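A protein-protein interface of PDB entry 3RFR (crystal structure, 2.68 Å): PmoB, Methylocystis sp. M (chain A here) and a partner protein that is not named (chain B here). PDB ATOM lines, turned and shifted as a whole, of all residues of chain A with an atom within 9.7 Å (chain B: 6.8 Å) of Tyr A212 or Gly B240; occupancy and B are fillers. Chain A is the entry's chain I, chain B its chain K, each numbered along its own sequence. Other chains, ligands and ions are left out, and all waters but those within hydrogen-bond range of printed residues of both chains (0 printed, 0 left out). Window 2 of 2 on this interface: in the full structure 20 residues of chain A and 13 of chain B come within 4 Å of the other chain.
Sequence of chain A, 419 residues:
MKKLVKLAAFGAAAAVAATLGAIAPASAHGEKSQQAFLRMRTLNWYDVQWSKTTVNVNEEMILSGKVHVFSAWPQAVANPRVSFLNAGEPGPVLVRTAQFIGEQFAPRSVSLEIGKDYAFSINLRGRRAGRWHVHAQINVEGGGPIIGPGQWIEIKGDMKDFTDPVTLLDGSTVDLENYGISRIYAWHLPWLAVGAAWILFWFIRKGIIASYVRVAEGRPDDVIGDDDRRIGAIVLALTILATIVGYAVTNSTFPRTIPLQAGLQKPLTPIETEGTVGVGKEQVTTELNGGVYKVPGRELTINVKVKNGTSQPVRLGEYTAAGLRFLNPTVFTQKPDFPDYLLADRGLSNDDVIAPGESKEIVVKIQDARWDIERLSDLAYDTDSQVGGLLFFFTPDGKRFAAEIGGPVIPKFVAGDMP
Printed residues of chain B within 4 Å of Ile A209: Leu B239.
Ala A210 touches none of the printed residues of chain B.
Of chain B, only Leu B236, Leu B239, Gly B240 and His B243 come within 4 Å of Tyr A212.
Of the printed residues of chain B, Ala A216 touches His B243.
Of the printed residues of chain B, Glu A217 touches His B243.
Of chain A, only Tyr A212 comes within 4 Å of Gly B240.
His B243 touches four residues of chain A.
The nearest residue of chain B that does not touch Tyr A212 is Arg B241 (5.9 Å).
Hydrophobic or aromatic side chains of chain B that line the printed part of chain A: Leu B236, Leu B239 and His B243.
Hydrophobic or aromatic side chains of chain A within 4 Å of the printed part of chain B: Ile A209, Tyr A212, Val A213 and Ala A216.
OE2 of Glu A217 lies within hydrogen-bond range of NE2 of His B243 (2.6 Å).
Among the printed residues, pairs that only touch across the chains: Ile A209 with Leu B239 (3.8 Å), Tyr A212 with Leu B236 (3.9 Å), Tyr A212 with Leu B239 (3.6 Å), Tyr A212 with Gly B240 (3.5 Å), Tyr A212 with His B243 (3.9 Å), Val A213 with His B243 (3.8 Å) and Ala A216 with His B243 (3.9 Å).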
ATOM      1  N   LYS A 206      16.959   9.549   2.716  1.00  0.00           N
ATOM      2  CA  LYS A 206      17.583   8.277   2.419  1.00  0.00           C
ATOM      3  C   LYS A 206      16.528   7.204   2.649  1.00  0.00           C
ATOM      4  O   LYS A 206      16.193   6.923   3.799  1.00  0.00           O
ATOM      5  CB  LYS A 206      18.905   8.089   3.265  1.00  0.00           C
ATOM      6  CG  LYS A 206      20.123   8.989   2.744  1.00  0.00           C
ATOM      7  CD  LYS A 206      20.795   8.408   1.444  1.00  0.00           C
ATOM      8  CE  LYS A 206      21.248   9.473   0.394  1.00  0.00           C
ATOM      9  NZ  LYS A 206      22.624  10.076   0.597  1.00  0.00           N
ATOM     10  N   GLY A 207      16.083   6.600   1.532  1.00  0.00           N
ATOM     11  CA  GLY A 207      14.716   6.079   1.327  1.00  0.00           C
ATOM     12  C   GLY A 207      14.541   4.584   1.466  1.00  0.00           C
ATOM     13  O   GLY A 207      15.340   3.907   2.164  1.00  0.00           O
ATOM     14  N   ILE A 208      13.499   4.053   0.816  1.00  0.00           N
ATOM     15  CA  ILE A 208      13.147   2.634   0.957  1.00  0.00           C
ATOM     16  C   ILE A 208      14.044   1.741   0.088  1.00  0.00           C
ATOM     17  O   ILE A 208      15.001   1.166   0.626  1.00  0.00           O
ATOM     18  CB  ILE A 208      11.630   2.355   0.786  1.00  0.00           C
ATOM     19  CG1 ILE A 208      10.829   2.991   1.936  1.00  0.00           C
ATOM     20  CG2 ILE A 208      11.316   0.831   0.721  1.00  0.00           C
ATOM     21  CD1 ILE A 208       9.299   2.947   1.754  1.00  0.00           C
ATOM     22  N   ILE A 209      13.783   1.640  -1.223  1.00  0.00           N
ATOM     23  CA  ILE A 209      14.737   0.991  -2.177  1.00  0.00           C
ATOM     24  C   ILE A 209      16.226   1.339  -1.958  1.00  0.00           C
ATOM     25  O   ILE A 209      17.037   0.450  -1.721  1.00  0.00           O
ATOM     26  CB  ILE A 209      14.381   1.236  -3.661  1.00  0.00           C
ATOM     27  CG1 ILE A 209      12.998   0.656  -3.974  1.00  0.00           C
ATOM     28  CG2 ILE A 209      15.418   0.574  -4.529  1.00  0.00           C
ATOM     29  CD1 ILE A 209      12.491   0.928  -5.349  1.00  0.00           C
ATOM     30  N   ALA A 210      16.593   2.612  -2.008  1.00  0.00           N
ATOM     31  CA  ALA A 210      17.978   2.977  -1.704  1.00  0.00           C
ATOM     32  C   ALA A 210      18.537   2.265  -0.422  1.00  0.00           C
ATOM     33  O   ALA A 210      19.695   1.819  -0.387  1.00  0.00           O
ATOM     34  CB  ALA A 210      18.183   4.526  -1.673  1.00  0.00           C
ATOM     35  N   SER A 211      17.680   2.100   0.584  1.00  0.00           N
ATOM     36  CA  SER A 211      18.082   1.471   1.865  1.00  0.00           C
ATOM     37  C   SER A 211      18.088  -0.075   1.856  1.00  0.00           C
ATOM     38  O   SER A 211      18.990  -0.703   2.488  1.00  0.00           O
ATOM     39  CB  SER A 211      17.199   1.991   3.011  1.00  0.00           C
ATOM     40  OG  SER A 211      17.780   3.151   3.614  1.00  0.00           O
ATOM     41  N   TYR A 212      17.081  -0.654   1.162  1.00  0.00           N
ATOM     42  CA  TYR A 212      17.026  -2.070   0.962  1.00  0.00           C
ATOM     43  C   TYR A 212      18.329  -2.459   0.329  1.00  0.00           C
ATOM     44  O   TYR A 212      19.077  -3.286   0.908  1.00  0.00           O
ATOM     45  CB  TYR A 212      15.912  -2.531   0.031  1.00  0.00           C
ATOM     46  CG  TYR A 212      16.050  -4.037  -0.273  1.00  0.00           C
ATOM     47  CD1 TYR A 212      15.605  -4.992   0.650  1.00  0.00           C
ATOM     48  CD2 TYR A 212      16.693  -4.500  -1.433  1.00  0.00           C
ATOM     49  CE1 TYR A 212      15.749  -6.354   0.415  1.00  0.00           C
ATOM     50  CE2 TYR A 212      16.833  -5.852  -1.672  1.00  0.00           C
ATOM     51  CZ  TYR A 212      16.363  -6.774  -0.736  1.00  0.00           C
ATOM     52  OH  TYR A 212      16.495  -8.126  -0.924  1.00  0.00           O
ATOM     53  N   VAL A 213      18.599  -1.874  -0.853  1.00  0.00           N
ATOM     54  CA  VAL A 213      19.872  -2.127  -1.553  1.00  0.00           C
ATOM     55  C   VAL A 213      21.104  -1.994  -0.617  1.00  0.00           C
ATOM     56  O   VAL A 213      21.874  -2.940  -0.513  1.00  0.00           O
ATOM     57  CB  VAL A 213      20.048  -1.342  -2.896  1.00  0.00           C
ATOM     58  CG1 VAL A 213      21.514  -1.443  -3.391  1.00  0.00           C
ATOM     59  CG2 VAL A 213      19.058  -1.844  -3.998  1.00  0.00           C
ATOM     60  N   ARG A 214      21.269  -0.889   0.108  1.00  0.00           N
ATOM     61  CA  ARG A 214      22.512  -0.749   0.910  1.00  0.00           C
ATOM     62  C   ARG A 214      22.730  -1.890   1.892  1.00  0.00           C
ATOM     63  O   ARG A 214      23.837  -2.415   2.008  1.00  0.00           O
ATOM     64  CB  ARG A 214      22.595   0.582   1.652  1.00  0.00           C
ATOM     65  CG  ARG A 214      22.895   1.711   0.775  1.00  0.00           C
ATOM     66  CD  ARG A 214      22.895   2.978   1.543  1.00  0.00           C
ATOM     67  NE  ARG A 214      22.653   4.095   0.634  1.00  0.00           N
ATOM     68  CZ  ARG A 214      23.038   5.345   0.863  1.00  0.00           C
ATOM     69  NH1 ARG A 214      23.708   5.646   1.988  1.00  0.00           N
ATOM     70  NH2 ARG A 214      22.766   6.287  -0.045  1.00  0.00           N
ATOM     71  N   VAL A 215      21.657  -2.265   2.586  1.00  0.00           N
ATOM     72  CA  VAL A 215      21.705  -3.309   3.611  1.00  0.00           C
ATOM     73  C   VAL A 215      22.001  -4.661   2.943  1.00  0.00           C
ATOM     74  O   VAL A 215      22.835  -5.437   3.427  1.00  0.00           O
ATOM     75  CB  VAL A 215      20.379  -3.353   4.438  1.00  0.00           C
ATOM     76  CG1 VAL A 215      20.136  -4.722   5.053  1.00  0.00           C
ATOM     77  CG2 VAL A 215      20.398  -2.279   5.517  1.00  0.00           C
ATOM     78  N   ALA A 216      21.331  -4.919   1.825  1.00  0.00           N
ATOM     79  CA  ALA A 216      21.455  -6.181   1.137  1.00  0.00           C
ATOM     80  C   ALA A 216      22.843  -6.328   0.524  1.00  0.00           C
ATOM     81  O   ALA A 216      23.346  -7.441   0.387  1.00  0.00           O
ATOM     82  CB  ALA A 216      20.360  -6.327   0.072  1.00  0.00           C
ATOM     83  N   GLU A 217      23.456  -5.200   0.162  1.00  0.00           N
ATOM     84  CA  GLU A 217      24.790  -5.191  -0.436  1.00  0.00           C
ATOM     85  C   GLU A 217      25.783  -5.296   0.699  1.00  0.00           C
ATOM     86  O   GLU A 217      25.675  -6.186   1.552  1.00  0.00           O
ATOM     87  CB  GLU A 217      25.033  -3.905  -1.231  1.00  0.00           C
ATOM     88  CG  GLU A 217      24.176  -3.751  -2.468  1.00  0.00           C
ATOM     89  CD  GLU A 217      24.833  -4.248  -3.728  1.00  0.00           C
ATOM     90  OE1 GLU A 217      26.074  -4.268  -3.796  1.00  0.00           O
ATOM     91  OE2 GLU A 217      24.110  -4.598  -4.674  1.00  0.00           O
ATOM     92  N   GLY A 218      26.744  -4.380   0.728  1.00  0.00           N
ATOM     93  CA  GLY A 218      27.658  -4.273   1.870  1.00  0.00           C
ATOM     94  C   GLY A 218      26.886  -4.025   3.149  1.00  0.00           C
ATOM     95  O   GLY A 218      25.704  -4.333   3.251  1.00  0.00           O
ATOM     96  N   ARG A 219      27.549  -3.462   4.133  1.00  0.00           N
ATOM     97  CA  ARG A 219      26.824  -3.094   5.331  1.00  0.00           C
ATOM     98  C   ARG A 219      25.831  -1.918   5.057  1.00  0.00           C
ATOM     99  O   ARG A 219      25.842  -1.293   3.965  1.00  0.00           O
ATOM    100  CB  ARG A 219      27.793  -2.865   6.536  1.00  0.00           C
ATOM    101  CG  ARG A 219      28.120  -4.180   7.330  1.00  0.00           C
ATOM    102  CD  ARG A 219      29.293  -4.053   8.355  1.00  0.00           C
ATOM    103  NE  ARG A 219      28.953  -3.243   9.540  1.00  0.00           N
ATOM    104  CZ  ARG A 219      29.823  -2.780  10.448  1.00  0.00           C
ATOM    105  NH1 ARG A 219      29.374  -2.056  11.462  1.00  0.00           N
ATOM    106  NH2 ARG A 219      31.133  -3.030  10.358  1.00  0.00           N
ATOM    107  N   PRO A 220      24.915  -1.677   6.014  1.00  0.00           N
ATOM    108  CA  PRO A 220      24.236  -0.402   6.200  1.00  0.00           C
ATOM    109  C   PRO A 220      25.251   0.711   6.389  1.00  0.00           C
ATOM    110  O   PRO A 220      25.919   1.097   5.418  1.00  0.00           O
ATOM    111  CB  PRO A 220      23.465  -0.598   7.509  1.00  0.00           C
ATOM    112  CG  PRO A 220      23.928  -1.921   8.075  1.00  0.00           C
ATOM    113  CD  PRO A 220      24.340  -2.720   6.877  1.00  0.00           C
ATOM    114  N   VAL A 223      23.588   3.877   5.758  1.00  0.00           N
ATOM    115  CA  VAL A 223      22.193   4.258   6.045  1.00  0.00           C
ATOM    116  C   VAL A 223      22.102   4.999   7.379  1.00  0.00           C
ATOM    117  O   VAL A 223      21.485   6.054   7.459  1.00  0.00           O
ATOM    118  CB  VAL A 223      21.242   3.043   6.095  1.00  0.00           C
ATOM    119  CG1 VAL A 223      19.809   3.511   6.187  1.00  0.00           C
ATOM    120  CG2 VAL A 223      21.430   2.136   4.892  1.00  0.00           C
ATOM    121  N   VAL B 235       6.794  -8.007  -0.145  1.00  0.00           N
ATOM    122  CA  VAL B 235       7.582  -6.858  -0.632  1.00  0.00           C
ATOM    123  C   VAL B 235       9.097  -7.113  -0.604  1.00  0.00           C
ATOM    124  O   VAL B 235       9.818  -6.566  -1.442  1.00  0.00           O
ATOM    125  CB  VAL B 235       7.219  -5.458  -0.040  1.00  0.00           C
ATOM    126  CG1 VAL B 235       5.760  -5.338   0.244  1.00  0.00           C
ATOM    127  CG2 VAL B 235       8.001  -5.165   1.193  1.00  0.00           C
ATOM    128  N   LEU B 236       9.585  -7.929   0.320  1.00  0.00           N
ATOM    129  CA  LEU B 236      11.001  -8.264   0.288  1.00  0.00           C
ATOM    130  C   LEU B 236      11.389  -9.085  -0.972  1.00  0.00           C
ATOM    131  O   LEU B 236      12.550  -9.026  -1.460  1.00  0.00           O
ATOM    132  CB  LEU B 236      11.403  -9.004   1.550  1.00  0.00           C
ATOM    133  CG  LEU B 236      11.527  -8.130   2.803  1.00  0.00           C
ATOM    134  CD1 LEU B 236      11.814  -8.957   4.027  1.00  0.00           C
ATOM    135  CD2 LEU B 236      12.604  -7.051   2.607  1.00  0.00           C
ATOM    136  N   GLN B 237      10.419  -9.839  -1.504  1.00  0.00           N
ATOM    137  CA  GLN B 237      10.702 -10.677  -2.642  1.00  0.00           C
ATOM    138  C   GLN B 237      10.738  -9.808  -3.872  1.00  0.00           C
ATOM    139  O   GLN B 237      11.603  -9.970  -4.730  1.00  0.00           O
ATOM    140  CB  GLN B 237       9.698 -11.809  -2.760  1.00  0.00           C
ATOM    141  CG  GLN B 237       9.928 -12.975  -1.758  1.00  0.00           C
ATOM    142  CD  GLN B 237       8.731 -13.926  -1.696  1.00  0.00           C
ATOM    143  OE1 GLN B 237       7.578 -13.541  -1.975  1.00  0.00           O
ATOM    144  NE2 GLN B 237       8.992 -15.161  -1.324  1.00  0.00           N
ATOM    145  N   ILE B 238       9.805  -8.866  -3.941  1.00  0.00           N
ATOM    146  CA  ILE B 238       9.821  -7.809  -4.957  1.00  0.00           C
ATOM    147  C   ILE B 238      11.148  -7.013  -4.870  1.00  0.00           C
ATOM    148  O   ILE B 238      11.910  -6.970  -5.834  1.00  0.00           O
ATOM    149  CB  ILE B 238       8.599  -6.903  -4.822  1.00  0.00           C
ATOM    150  CG1 ILE B 238       7.329  -7.648  -5.287  1.00  0.00           C
ATOM    151  CG2 ILE B 238       8.827  -5.641  -5.589  1.00  0.00           C
ATOM    152  CD1 ILE B 238       6.051  -6.939  -4.968  1.00  0.00           C
ATOM    153  N   LEU B 239      11.475  -6.443  -3.717  1.00  0.00           N
ATOM    154  CA  LEU B 239      12.796  -5.835  -3.580  1.00  0.00           C
ATOM    155  C   LEU B 239      14.021  -6.741  -3.957  1.00  0.00           C
ATOM    156  O   LEU B 239      14.912  -6.285  -4.693  1.00  0.00           O
ATOM    157  CB  LEU B 239      12.964  -5.193  -2.209  1.00  0.00           C
ATOM    158  CG  LEU B 239      11.948  -4.076  -1.949  1.00  0.00           C
ATOM    159  CD1 LEU B 239      12.000  -3.667  -0.487  1.00  0.00           C
ATOM    160  CD2 LEU B 239      12.143  -2.871  -2.869  1.00  0.00           C
ATOM    161  N   GLY B 240      14.066  -7.993  -3.471  1.00  0.00           N
ATOM    162  CA  GLY B 240      15.013  -9.014  -3.986  1.00  0.00           C
ATOM    163  C   GLY B 240      15.122  -8.950  -5.522  1.00  0.00           C
ATOM    164  O   GLY B 240      16.227  -9.024  -6.090  1.00  0.00           O
ATOM    165  N   ARG B 241      13.980  -8.752  -6.198  1.00  0.00           N
ATOM    166  CA  ARG B 241      13.866  -8.842  -7.657  1.00  0.00           C
ATOM    167  C   ARG B 241      14.177  -7.511  -8.364  1.00  0.00           C
ATOM    168  O   ARG B 241      14.748  -7.473  -9.461  1.00  0.00           O
ATOM    169  CB  ARG B 241      12.444  -9.272  -7.960  1.00  0.00           C
ATOM    170  CG  ARG B 241      12.227  -9.952  -9.267  1.00  0.00           C
ATOM    171  CD  ARG B 241      12.852 -11.344  -9.370  1.00  0.00           C
ATOM    172  NE  ARG B 241      13.223 -11.579 -10.768  1.00  0.00           N
ATOM    173  CZ  ARG B 241      14.467 -11.596 -11.241  1.00  0.00           C
ATOM    174  NH1 ARG B 241      15.520 -11.462 -10.430  1.00  0.00           N
ATOM    175  NH2 ARG B 241      14.653 -11.776 -12.546  1.00  0.00           N
ATOM    176  N   ILE B 242      13.790  -6.407  -7.731  1.00  0.00           N
ATOM    177  CA  ILE B 242      14.190  -5.072  -8.185  1.00  0.00           C
ATOM    178  C   ILE B 242      15.701  -4.884  -8.091  1.00  0.00           C
ATOM    179  O   ILE B 242      16.301  -4.292  -8.952  1.00  0.00           O
ATOM    180  CB  ILE B 242      13.452  -3.963  -7.380  1.00  0.00           C
ATOM    181  CG1 ILE B 242      12.021  -3.846  -7.889  1.00  0.00           C
ATOM    182  CG2 ILE B 242      14.172  -2.603  -7.509  1.00  0.00           C
ATOM    183  CD1 ILE B 242      11.162  -2.966  -7.080  1.00  0.00           C
ATOM    184  N   HIS B 243      16.295  -5.411  -7.029  1.00  0.00           N
ATOM    185  CA  HIS B 243      17.716  -5.292  -6.781  1.00  0.00           C
ATOM    186  C   HIS B 243      18.509  -5.941  -7.897  1.00  0.00           C
ATOM    187  O   HIS B 243      19.560  -5.443  -8.302  1.00  0.00           O
ATOM    188  CB  HIS B 243      18.033  -5.948  -5.441  1.00  0.00           C
ATOM    189  CG  HIS B 243      19.447  -5.785  -5.002  1.00  0.00           C
ATOM    190  ND1 HIS B 243      19.964  -6.475  -3.932  1.00  0.00           N
ATOM    191  CD2 HIS B 243      20.456  -5.029  -5.489  1.00  0.00           C
ATOM    192  CE1 HIS B 243      21.233  -6.144  -3.771  1.00  0.00           C
ATOM    193  NE2 HIS B 243      21.555  -5.270  -4.708  1.00  0.00           N
ATOM    194  N   ALA B 244      17.975  -7.046  -8.403  1.00  0.00           N
ATOM    195  CA  ALA B 244      18.694  -7.878  -9.348  1.00  0.00           C
ATOM    196  C   ALA B 244      18.525  -7.353 -10.754  1.00  0.00           C
ATOM    197  O   ALA B 244      19.355  -7.631 -11.631  1.00  0.00           O
ATOM    198  CB  ALA B 244      18.233  -9.303  -9.253  1.00  0.00           C
ATOM    199  N   LEU B 245      17.463  -6.586 -10.980  1.00  0.00           N
ATOM    200  CA  LEU B 245      17.317  -5.943 -12.280  1.00  0.00           C
ATOM    201  C   LEU B 245      18.135  -4.646 -12.419  1.00  0.00           C
ATOM    202  O   LEU B 245      17.636  -3.681 -12.949  1.00  0.00           O
ATOM    203  CB  LEU B 245      15.849  -5.741 -12.669  1.00  0.00           C
ATOM    204  CG  LEU B 245      14.989  -6.996 -12.737  1.00  0.00           C
ATOM    205  CD1 LEU B 245      13.637  -6.692 -13.342  1.00  0.00           C
ATOM    206  CD2 LEU B 245      15.672  -8.063 -13.539  1.00  0.00           C
